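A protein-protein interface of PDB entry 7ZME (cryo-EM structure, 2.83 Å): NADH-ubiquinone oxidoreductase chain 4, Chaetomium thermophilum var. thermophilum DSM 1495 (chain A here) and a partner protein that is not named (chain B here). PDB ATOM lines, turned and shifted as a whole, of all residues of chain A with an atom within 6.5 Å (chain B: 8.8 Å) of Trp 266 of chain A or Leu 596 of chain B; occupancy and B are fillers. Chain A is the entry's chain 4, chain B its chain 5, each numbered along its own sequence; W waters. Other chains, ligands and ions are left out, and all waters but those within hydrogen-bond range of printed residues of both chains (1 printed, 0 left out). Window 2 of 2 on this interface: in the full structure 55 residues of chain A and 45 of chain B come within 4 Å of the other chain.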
ATOM      1  N   ALA A 260      24.569 -28.769 -14.635  1.00  0.00           N
ATOM      2  CA  ALA A 260      25.164 -27.454 -14.844  1.00  0.00           C
ATOM      3  C   ALA A 260      24.240 -26.545 -15.638  1.00  0.00           C
ATOM      4  O   ALA A 260      24.232 -25.329 -15.420  1.00  0.00           O
ATOM      5  CB  ALA A 260      26.510 -27.582 -15.551  1.00  0.00           C
ATOM      6  N   PRO A 264      21.308 -22.827 -12.632  1.00  0.00           N
ATOM      7  CA  PRO A 264      22.231 -22.853 -13.771  1.00  0.00           C
ATOM      8  C   PRO A 264      23.571 -22.224 -13.412  1.00  0.00           C
ATOM      9  O   PRO A 264      23.625 -21.338 -12.562  1.00  0.00           O
ATOM     10  CB  PRO A 264      21.501 -22.023 -14.818  1.00  0.00           C
ATOM     11  CG  PRO A 264      20.793 -21.004 -14.016  1.00  0.00           C
ATOM     12  CD  PRO A 264      20.410 -21.663 -12.710  1.00  0.00           C
ATOM     13  N   VAL A 265      24.637 -22.681 -14.045  1.00  0.00           N
ATOM     14  CA  VAL A 265      25.949 -22.084 -13.852  1.00  0.00           C
ATOM     15  C   VAL A 265      26.130 -20.973 -14.877  1.00  0.00           C
ATOM     16  O   VAL A 265      25.442 -20.920 -15.897  1.00  0.00           O
ATOM     17  CB  VAL A 265      27.071 -23.136 -13.957  1.00  0.00           C
ATOM     18  CG1 VAL A 265      26.806 -24.280 -12.999  1.00  0.00           C
ATOM     19  CG2 VAL A 265      27.196 -23.645 -15.380  1.00  0.00           C
ATOM     20  N   TRP A 266      27.061 -20.065 -14.600  1.00  0.00           N
ATOM     21  CA  TRP A 266      27.268 -18.934 -15.490  1.00  0.00           C
ATOM     22  C   TRP A 266      27.779 -19.405 -16.845  1.00  0.00           C
ATOM     23  O   TRP A 266      28.554 -20.360 -16.940  1.00  0.00           O
ATOM     24  CB  TRP A 266      28.251 -17.933 -14.887  1.00  0.00           C
ATOM     25  CG  TRP A 266      28.301 -16.681 -15.684  1.00  0.00           C
ATOM     26  CD1 TRP A 266      27.540 -15.571 -15.505  1.00  0.00           C
ATOM     27  CD2 TRP A 266      29.122 -16.424 -16.829  1.00  0.00           C
ATOM     28  NE1 TRP A 266      27.848 -14.628 -16.452  1.00  0.00           N
ATOM     29  CE2 TRP A 266      28.816 -15.131 -17.278  1.00  0.00           C
ATOM     30  CE3 TRP A 266      30.092 -17.163 -17.512  1.00  0.00           C
ATOM     31  CZ2 TRP A 266      29.443 -14.558 -18.377  1.00  0.00           C
ATOM     32  CZ3 TRP A 266      30.710 -16.595 -18.601  1.00  0.00           C
ATOM     33  CH2 TRP A 266      30.388 -15.306 -19.022  1.00  0.00           C
ATOM     34  N   GLY A 267      27.340 -18.723 -17.900  1.00  0.00           N
ATOM     35  CA  GLY A 267      27.640 -19.113 -19.253  1.00  0.00           C
ATOM     36  C   GLY A 267      26.641 -20.075 -19.853  1.00  0.00           C
ATOM     37  O   GLY A 267      26.602 -20.229 -21.077  1.00  0.00           O
ATOM     38  N   LEU A 268      25.834 -20.727 -19.018  1.00  0.00           N
ATOM     39  CA  LEU A 268      24.750 -21.596 -19.453  1.00  0.00           C
ATOM     40  C   LEU A 268      23.410 -21.109 -18.923  1.00  0.00           C
ATOM     41  O   LEU A 268      22.442 -21.871 -18.892  1.00  0.00           O
ATOM     42  CB  LEU A 268      25.003 -23.035 -19.004  1.00  0.00           C
ATOM     43  CG  LEU A 268      25.668 -23.993 -19.991  1.00  0.00           C
ATOM     44  CD1 LEU A 268      24.754 -24.238 -21.173  1.00  0.00           C
ATOM     45  CD2 LEU A 268      27.014 -23.462 -20.447  1.00  0.00           C
ATOM     46  N   ASN A 269      23.340 -19.842 -18.515  1.00  0.00           N
ATOM     47  CA  ASN A 269      22.225 -19.308 -17.748  1.00  0.00           C
ATOM     48  C   ASN A 269      21.346 -18.353 -18.545  1.00  0.00           C
ATOM     49  O   ASN A 269      20.506 -17.669 -17.953  1.00  0.00           O
ATOM     50  CB  ASN A 269      22.753 -18.607 -16.495  1.00  0.00           C
ATOM     51  CG  ASN A 269      23.666 -17.438 -16.819  1.00  0.00           C
ATOM     52  OD1 ASN A 269      24.760 -17.613 -17.352  1.00  0.00           O
ATOM     53  ND2 ASN A 269      23.212 -16.237 -16.511  1.00  0.00           N
ATOM     54  N   ILE A 321      34.015 -23.602 -11.759  1.00  0.00           N
ATOM     55  CA  ILE A 321      32.779 -23.091 -12.343  1.00  0.00           C
ATOM     56  C   ILE A 321      31.958 -22.356 -11.294  1.00  0.00           C
ATOM     57  O   ILE A 321      31.422 -21.274 -11.552  1.00  0.00           O
ATOM     58  CB  ILE A 321      31.984 -24.241 -12.987  1.00  0.00           C
ATOM     59  CG1 ILE A 321      32.795 -24.884 -14.111  1.00  0.00           C
ATOM     60  CG2 ILE A 321      30.651 -23.747 -13.506  1.00  0.00           C
ATOM     61  CD1 ILE A 321      32.456 -26.334 -14.351  1.00  0.00           C
ATOM     62  N   ILE A 324      33.673 -18.993 -10.376  1.00  0.00           N
ATOM     63  CA  ILE A 324      33.476 -18.118 -11.526  1.00  0.00           C
ATOM     64  C   ILE A 324      32.024 -17.674 -11.604  1.00  0.00           C
ATOM     65  O   ILE A 324      31.730 -16.517 -11.924  1.00  0.00           O
ATOM     66  CB  ILE A 324      33.925 -18.829 -12.817  1.00  0.00           C
ATOM     67  CG1 ILE A 324      35.450 -18.844 -12.916  1.00  0.00           C
ATOM     68  CG2 ILE A 324      33.307 -18.183 -14.046  1.00  0.00           C
ATOM     69  CD1 ILE A 324      36.054 -17.504 -13.205  1.00  0.00           C
ATOM     70  N   THR A 325      31.093 -18.583 -11.305  1.00  0.00           N
ATOM     71  CA  THR A 325      29.680 -18.226 -11.351  1.00  0.00           C
ATOM     72  C   THR A 325      29.340 -17.185 -10.296  1.00  0.00           C
ATOM     73  O   THR A 325      28.621 -16.224 -10.580  1.00  0.00           O
ATOM     74  CB  THR A 325      28.807 -19.466 -11.176  1.00  0.00           C
ATOM     75  OG1 THR A 325      29.172 -20.448 -12.154  1.00  0.00           O
ATOM     76  CG2 THR A 325      27.339 -19.109 -11.347  1.00  0.00           C
ATOM     77  N   VAL A 326      29.860 -17.344  -9.078  1.00  0.00           N
ATOM     78  CA  VAL A 326      29.551 -16.391  -8.014  1.00  0.00           C
ATOM     79  C   VAL A 326      30.008 -14.992  -8.407  1.00  0.00           C
ATOM     80  O   VAL A 326      29.260 -14.016  -8.280  1.00  0.00           O
ATOM     81  CB  VAL A 326      30.186 -16.839  -6.684  1.00  0.00           C
ATOM     82  CG1 VAL A 326      30.214 -15.685  -5.690  1.00  0.00           C
ATOM     83  CG2 VAL A 326      29.424 -18.010  -6.101  1.00  0.00           C
ATOM     84  N   TYR A 328      30.850 -13.749 -11.525  1.00  0.00           N
ATOM     85  CA  TYR A 328      30.251 -13.210 -12.739  1.00  0.00           C
ATOM     86  C   TYR A 328      28.765 -12.939 -12.551  1.00  0.00           C
ATOM     87  O   TYR A 328      28.246 -11.933 -13.044  1.00  0.00           O
ATOM     88  CB  TYR A 328      30.475 -14.163 -13.910  1.00  0.00           C
ATOM     89  CG  TYR A 328      31.908 -14.278 -14.362  1.00  0.00           C
ATOM     90  CD1 TYR A 328      32.934 -13.637 -13.679  1.00  0.00           C
ATOM     91  CD2 TYR A 328      32.240 -15.030 -15.476  1.00  0.00           C
ATOM     92  CE1 TYR A 328      34.245 -13.748 -14.091  1.00  0.00           C
ATOM     93  CE2 TYR A 328      33.546 -15.143 -15.893  1.00  0.00           C
ATOM     94  CZ  TYR A 328      34.544 -14.501 -15.197  1.00  0.00           C
ATOM     95  OH  TYR A 328      35.845 -14.611 -15.613  1.00  0.00           O
ATOM     96  N   ALA A 329      28.063 -13.826 -11.844  1.00  0.00           N
ATOM     97  CA  ALA A 329      26.641 -13.606 -11.615  1.00  0.00           C
ATOM     98  C   ALA A 329      26.398 -12.424 -10.689  1.00  0.00           C
ATOM     99  O   ALA A 329      25.282 -11.904 -10.640  1.00  0.00           O
ATOM    100  CB  ALA A 329      25.980 -14.862 -11.051  1.00  0.00           C
ATOM    101  N   SER A 332      27.263  -8.807 -12.877  1.00  0.00           N
ATOM    102  CA  SER A 332      26.236  -8.507 -13.867  1.00  0.00           C
ATOM    103  C   SER A 332      24.945  -8.038 -13.209  1.00  0.00           C
ATOM    104  O   SER A 332      24.318  -7.082 -13.677  1.00  0.00           O
ATOM    105  CB  SER A 332      25.978  -9.727 -14.745  1.00  0.00           C
ATOM    106  OG  SER A 332      27.047  -9.954 -15.639  1.00  0.00           O
ATOM    107  N   TYR A 345      18.596 -13.196 -11.492  1.00  0.00           N
ATOM    108  CA  TYR A 345      19.982 -13.539 -11.744  1.00  0.00           C
ATOM    109  C   TYR A 345      20.810 -13.573 -10.470  1.00  0.00           C
ATOM    110  O   TYR A 345      21.932 -14.089 -10.486  1.00  0.00           O
ATOM    111  CB  TYR A 345      20.542 -12.559 -12.773  1.00  0.00           C
ATOM    112  CG  TYR A 345      21.958 -12.781 -13.216  1.00  0.00           C
ATOM    113  CD1 TYR A 345      22.261 -13.810 -14.086  1.00  0.00           C
ATOM    114  CD2 TYR A 345      22.950 -11.888 -12.906  1.00  0.00           C
ATOM    115  CE1 TYR A 345      23.526 -14.007 -14.546  1.00  0.00           C
ATOM    116  CE2 TYR A 345      24.219 -12.073 -13.375  1.00  0.00           C
ATOM    117  CZ  TYR A 345      24.504 -13.138 -14.199  1.00  0.00           C
ATOM    118  OH  TYR A 345      25.770 -13.346 -14.683  1.00  0.00           O
ATOM    119  N   VAL A 348      21.086 -17.255  -9.622  1.00  0.00           N
ATOM    120  CA  VAL A 348      22.263 -17.890 -10.204  1.00  0.00           C
ATOM    121  C   VAL A 348      23.443 -17.791  -9.250  1.00  0.00           C
ATOM    122  O   VAL A 348      24.256 -18.716  -9.154  1.00  0.00           O
ATOM    123  CB  VAL A 348      22.571 -17.247 -11.571  1.00  0.00           C
ATOM    124  CG1 VAL A 348      23.837 -17.822 -12.185  1.00  0.00           C
ATOM    125  CG2 VAL A 348      21.386 -17.410 -12.510  1.00  0.00           C
ATOM    126  N   LEU B 588      33.560  -3.908 -14.627  1.00  0.00           N
ATOM    127  CA  LEU B 588      33.622  -5.346 -14.862  1.00  0.00           C
ATOM    128  C   LEU B 588      32.239  -5.911 -15.136  1.00  0.00           C
ATOM    129  O   LEU B 588      32.065  -6.725 -16.047  1.00  0.00           O
ATOM    130  CB  LEU B 588      34.250  -6.065 -13.672  1.00  0.00           C
ATOM    131  CG  LEU B 588      35.738  -5.896 -13.418  1.00  0.00           C
ATOM    132  CD1 LEU B 588      36.096  -6.614 -12.137  1.00  0.00           C
ATOM    133  CD2 LEU B 588      36.531  -6.437 -14.580  1.00  0.00           C
ATOM    134  N   GLY B 589      31.244  -5.492 -14.354  1.00  0.00           N
ATOM    135  CA  GLY B 589      29.881  -5.900 -14.633  1.00  0.00           C
ATOM    136  C   GLY B 589      29.430  -5.494 -16.020  1.00  0.00           C
ATOM    137  O   GLY B 589      28.790  -6.274 -16.726  1.00  0.00           O
ATOM    138  N   GLY B 590      29.782  -4.278 -16.441  1.00  0.00           N
ATOM    139  CA  GLY B 590      29.413  -3.829 -17.773  1.00  0.00           C
ATOM    140  C   GLY B 590      29.988  -4.704 -18.869  1.00  0.00           C
ATOM    141  O   GLY B 590      29.322  -4.978 -19.869  1.00  0.00           O
ATOM    142  N   GLN B 591      31.234  -5.153 -18.701  1.00  0.00           N
ATOM    143  CA  GLN B 591      31.835  -6.057 -19.675  1.00  0.00           C
ATOM    144  C   GLN B 591      31.049  -7.358 -19.774  1.00  0.00           C
ATOM    145  O   GLN B 591      30.803  -7.866 -20.873  1.00  0.00           O
ATOM    146  CB  GLN B 591      33.287  -6.347 -19.298  1.00  0.00           C
ATOM    147  CG  GLN B 591      34.138  -5.127 -19.025  1.00  0.00           C
ATOM    148  CD  GLN B 591      34.890  -4.648 -20.239  1.00  0.00           C
ATOM    149  OE1 GLN B 591      34.305  -4.405 -21.289  1.00  0.00           O
ATOM    150  NE2 GLN B 591      36.202  -4.510 -20.103  1.00  0.00           N
ATOM    151  N   ILE B 592      30.651  -7.919 -18.630  1.00  0.00           N
ATOM    152  CA  ILE B 592      29.967  -9.209 -18.630  1.00  0.00           C
ATOM    153  C   ILE B 592      28.567  -9.086 -19.217  1.00  0.00           C
ATOM    154  O   ILE B 592      28.145  -9.925 -20.019  1.00  0.00           O
ATOM    155  CB  ILE B 592      29.937  -9.798 -17.209  1.00  0.00           C
ATOM    156  CG1 ILE B 592      31.304  -9.671 -16.546  1.00  0.00           C
ATOM    157  CG2 ILE B 592      29.495 -11.251 -17.235  1.00  0.00           C
ATOM    158  CD1 ILE B 592      31.304 -10.057 -15.093  1.00  0.00           C
ATOM    159  N   THR B 593      27.820  -8.051 -18.823  1.00  0.00           N
ATOM    160  CA  THR B 593      26.455  -7.894 -19.321  1.00  0.00           C
ATOM    161  C   THR B 593      26.419  -7.632 -20.820  1.00  0.00           C
ATOM    162  O   THR B 593      25.566  -8.178 -21.528  1.00  0.00           O
ATOM    163  CB  THR B 593      25.738  -6.766 -18.579  1.00  0.00           C
ATOM    164  OG1 THR B 593      26.271  -5.501 -18.992  1.00  0.00           O
ATOM    165  CG2 THR B 593      25.861  -6.926 -17.082  1.00  0.00           C
ATOM    166  N   LYS B 594      27.325  -6.796 -21.324  1.00  0.00           N
ATOM    167  CA  LYS B 594      27.241  -6.341 -22.706  1.00  0.00           C
ATOM    168  C   LYS B 594      28.039  -7.218 -23.663  1.00  0.00           C
ATOM    169  O   LYS B 594      27.550  -7.566 -24.741  1.00  0.00           O
ATOM    170  CB  LYS B 594      27.704  -4.886 -22.803  1.00  0.00           C
ATOM    171  CG  LYS B 594      26.866  -3.937 -21.971  1.00  0.00           C
ATOM    172  CD  LYS B 594      27.338  -2.498 -22.091  1.00  0.00           C
ATOM    173  CE  LYS B 594      28.725  -2.316 -21.505  1.00  0.00           C
ATOM    174  NZ  LYS B 594      28.942  -0.933 -20.997  1.00  0.00           N
ATOM    175  N   ILE B 595      29.264  -7.584 -23.295  1.00  0.00           N
ATOM    176  CA  ILE B 595      30.104  -8.359 -24.199  1.00  0.00           C
ATOM    177  C   ILE B 595      29.951  -9.866 -24.012  1.00  0.00           C
ATOM    178  O   ILE B 595      30.109 -10.618 -24.985  1.00  0.00           O
ATOM    179  CB  ILE B 595      31.579  -7.948 -24.040  1.00  0.00           C
ATOM    180  CG1 ILE B 595      31.724  -6.441 -24.200  1.00  0.00           C
ATOM    181  CG2 ILE B 595      32.460  -8.654 -25.046  1.00  0.00           C
ATOM    182  CD1 ILE B 595      33.031  -5.918 -23.689  1.00  0.00           C
ATOM    183  N   LEU B 596      29.634 -10.332 -22.806  1.00  0.00           N
ATOM    184  CA  LEU B 596      29.543 -11.765 -22.540  1.00  0.00           C
ATOM    185  C   LEU B 596      28.097 -12.247 -22.538  1.00  0.00           C
ATOM    186  O   LEU B 596      27.726 -13.060 -23.383  1.00  0.00           O
ATOM    187  CB  LEU B 596      30.238 -12.112 -21.221  1.00  0.00           C
ATOM    188  CG  LEU B 596      31.742 -12.382 -21.282  1.00  0.00           C
ATOM    189  CD1 LEU B 596      31.993 -13.573 -22.173  1.00  0.00           C
ATOM    190  CD2 LEU B 596      32.529 -11.183 -21.766  1.00  0.00           C
ATOM    191  N   ASP B 597      27.286 -11.789 -21.594  1.00  0.00           N
ATOM    192  CA  ASP B 597      25.934 -12.367 -21.393  1.00  0.00           C
ATOM    193  C   ASP B 597      24.918 -11.859 -22.408  1.00  0.00           C
ATOM    194  O   ASP B 597      23.888 -12.516 -22.562  1.00  0.00           O
ATOM    195  CB  ASP B 597      25.465 -12.069 -19.968  1.00  0.00           C
ATOM    196  CG  ASP B 597      25.863 -13.104 -18.941  1.00  0.00           C
ATOM    197  OD1 ASP B 597      26.353 -14.174 -19.350  1.00  0.00           O
ATOM    198  OD2 ASP B 597      25.662 -12.833 -17.743  1.00  0.00           O
ATOM    199  N   LYS B 598      25.173 -10.748 -23.077  1.00  0.00           N
ATOM    200  CA  LYS B 598      24.292 -10.297 -24.180  1.00  0.00           C
ATOM    201  C   LYS B 598      25.196 -10.159 -25.399  1.00  0.00           C
ATOM    202  O   LYS B 598      24.962  -9.241 -26.197  1.00  0.00           O
ATOM    203  CB  LYS B 598      23.582  -8.998 -23.809  1.00  0.00           C
ATOM    204  CG  LYS B 598      22.575  -9.110 -22.673  1.00  0.00           C
ATOM    205  CD  LYS B 598      21.941  -7.793 -22.296  1.00  0.00           C
ATOM    206  CE  LYS B 598      21.168  -7.860 -20.997  1.00  0.00           C
ATOM    207  NZ  LYS B 598      20.189  -8.973 -20.995  1.00  0.00           N
ATOM    208  N   GLY B 599      26.230 -11.003 -25.488  1.00  0.00           N
ATOM    209  CA  GLY B 599      27.224 -10.881 -26.566  1.00  0.00           C
ATOM    210  C   GLY B 599      27.721 -12.208 -27.082  1.00  0.00           C
ATOM    211  O   GLY B 599      27.002 -12.823 -27.875  1.00  0.00           O
ATOM    212  N   SER B 600      28.928 -12.612 -26.696  1.00  0.00           N
ATOM    213  CA  SER B 600      29.508 -13.831 -27.247  1.00  0.00           C
ATOM    214  C   SER B 600      28.788 -15.089 -26.773  1.00  0.00           C
ATOM    215  O   SER B 600      28.701 -16.070 -27.520  1.00  0.00           O
ATOM    216  CB  SER B 600      30.983 -13.893 -26.879  1.00  0.00           C
ATOM    217  OG  SER B 600      31.153 -13.881 -25.477  1.00  0.00           O
ATOM    218  N   ILE B 601      28.291 -15.104 -25.533  1.00  0.00           N
ATOM    219  CA  ILE B 601      27.576 -16.286 -25.057  1.00  0.00           C
ATOM    220  C   ILE B 601      26.335 -16.524 -25.903  1.00  0.00           C
ATOM    221  O   ILE B 601      25.991 -17.670 -26.219  1.00  0.00           O
ATOM    222  CB  ILE B 601      27.229 -16.155 -23.561  1.00  0.00           C
ATOM    223  CG1 ILE B 601      28.498 -16.015 -22.712  1.00  0.00           C
ATOM    224  CG2 ILE B 601      26.402 -17.342 -23.094  1.00  0.00           C
ATOM    225  CD1 ILE B 601      29.149 -17.312 -22.344  1.00  0.00           C
ATOM    226  N   GLU B 602      25.648 -15.449 -26.293  1.00  0.00           N
ATOM    227  CA  GLU B 602      24.529 -15.577 -27.218  1.00  0.00           C
ATOM    228  C   GLU B 602      24.996 -15.977 -28.614  1.00  0.00           C
ATOM    229  O   GLU B 602      24.393 -16.849 -29.245  1.00  0.00           O
ATOM    230  CB  GLU B 602      23.741 -14.267 -27.274  1.00  0.00           C
ATOM    231  CG  GLU B 602      22.820 -14.008 -26.088  1.00  0.00           C
ATOM    232  CD  GLU B 602      21.632 -14.961 -26.011  1.00  0.00           C
ATOM    233  OE1 GLU B 602      20.778 -14.767 -25.122  1.00  0.00           O
ATOM    234  OE2 GLU B 602      21.519 -15.879 -26.847  1.00  0.00           O
ATOM    235  N   LEU B 603      26.061 -15.348 -29.116  1.00  0.00           N
ATOM    236  CA  LEU B 603      26.506 -15.631 -30.477  1.00  0.00           C
ATOM    237  C   LEU B 603      27.158 -16.999 -30.592  1.00  0.00           C
ATOM    238  O   LEU B 603      26.860 -17.751 -31.523  1.00  0.00           O
ATOM    239  CB  LEU B 603      27.472 -14.557 -30.967  1.00  0.00           C
ATOM    240  CG  LEU B 603      27.868 -14.788 -32.424  1.00  0.00           C
ATOM    241  CD1 LEU B 603      26.655 -14.609 -33.313  1.00  0.00           C
ATOM    242  CD2 LEU B 603      28.983 -13.871 -32.860  1.00  0.00           C
ATOM    243  N   PHE B 604      28.056 -17.343 -29.676  1.00  0.00           N
ATOM    244  CA  PHE B 604      28.614 -18.693 -29.661  1.00  0.00           C
ATOM    245  C   PHE B 604      27.732 -19.587 -28.788  1.00  0.00           C
ATOM    246  O   PHE B 604      28.124 -20.106 -27.747  1.00  0.00           O
ATOM    247  CB  PHE B 604      30.064 -18.669 -29.192  1.00  0.00           C
ATOM    248  CG  PHE B 604      30.716 -20.021 -29.173  1.00  0.00           C
ATOM    249  CD1 PHE B 604      30.995 -20.676 -30.356  1.00  0.00           C
ATOM    250  CD2 PHE B 604      31.069 -20.624 -27.980  1.00  0.00           C
ATOM    251  CE1 PHE B 604      31.596 -21.917 -30.353  1.00  0.00           C
ATOM    252  CE2 PHE B 604      31.671 -21.862 -27.970  1.00  0.00           C
ATOM    253  CZ  PHE B 604      31.936 -22.510 -29.158  1.00  0.00           C
HETATM  254  O   HOH W   1      23.047 -15.094 -19.801  1.00  0.00           O
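OD2 of Asp 597 of chain B sits at hydrogen-bond distance from NE1 of Trp 266 of chain A (3.1 Å).
The side-chain carboxylate (OD2) of Asp 597 of chain B lies within hydrogen-bond range of the side-chain hydroxyl (OH) of Tyr 345 of chain A, at 3.1 Å.
O of Tyr 328 of chain A is in hydrogen-bond range of OG of Ser 332 of chain A (3.5 Å).
The backbone carbonyl oxygen of Tyr 328 of chain A is in hydrogen-bond range of the side-chain hydroxyl of Tyr 345 of chain A (3.3 Å).
The side-chain hydroxyl (OG1) of Thr 593 of chain B sits close to the backbone carbonyl oxygen (O) of Gly 589 of chain B (3.5 Å).
The backbone carbonyl oxygen (O) of Gln 591 of chain B is in hydrogen-bond range of the backbone NH (N) of Leu 596 of chain B, 3.3 Å away.
O of Ile 592 of chain B sits at hydrogen-bond distance from N of Asp 597 of chain B, 2.6 Å away.
The backbone NH of Lys 598 of chain B lies within hydrogen-bond range of the backbone carbonyl oxygen of Thr 593 of chain B (3.0 Å).
Among the printed residues, merely in contact across the chains: Ser 332 of chain A with Ile 592 of chain B (3.2 Å), Trp 266 of chain A with Ile 592 of chain B (3.5 Å), Gly 267 of chain A with Ile 601 of chain B (3.5 Å), Ser 332 of chain A with Thr 593 of chain B (3.6 Å), Ser 332 of chain A with Asp 597 of chain B (3.8 Å) and Trp 266 of chain A with Leu 596 of chain B (3.8 Å).
No residue of chain B comes within 4 Å of Val 265 of chain A.
Trp 266 of chain A touches three residues of chain B.
Gly 267 of chain A touches one residue of chain B.
Of the printed residues of chain B, Tyr 345 of chain A touches Asp 597 (3.1 Å).
Printed residues of chain A within 4 Å of Ile 592 of chain B: Trp 266 and Ser 332.
Of the printed residues of chain A, Thr 593 of chain B touches Ser 332 (3.6 Å).
Leu 596 of chain B touches just one residue of chain A: Trp 266 (3.8 Å).
Of the printed residues of chain A, Asp 597 of chain B touches Trp 266 (3.1 Å), Ser 332 (3.8 Å) and Tyr 345 (3.1 Å).
Lys 598 of chain B touches none of the printed residues of chain A.
Of the printed residues of chain A, Ile 601 of chain B touches Gly 267.
The nearest residue of chain B that does not touch Trp 266 of chain A is Ile 601 of chain B (4.1 Å).
The nearest residue of chain A that does not touch Leu 596 of chain B is Tyr 328 of chain A (6.3 Å).
Of the 17 printed residues of chain B, 5 touch a printed residue of chain A.
Of the 16 printed residues of chain A, 4 touch a printed residue of chain B.
Hydrophobic or aromatic side chains of chain A that line the printed part of chain B: Trp 266 and Tyr 345.
Water W1 lies within hydrogen-bond range of the side-chain carboxylate (OD1) of Asp 597 of chain B (3.5 Å) and the side-chain amide nitrogen (ND2) of Asn 269 of chain A (3.5 Å).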
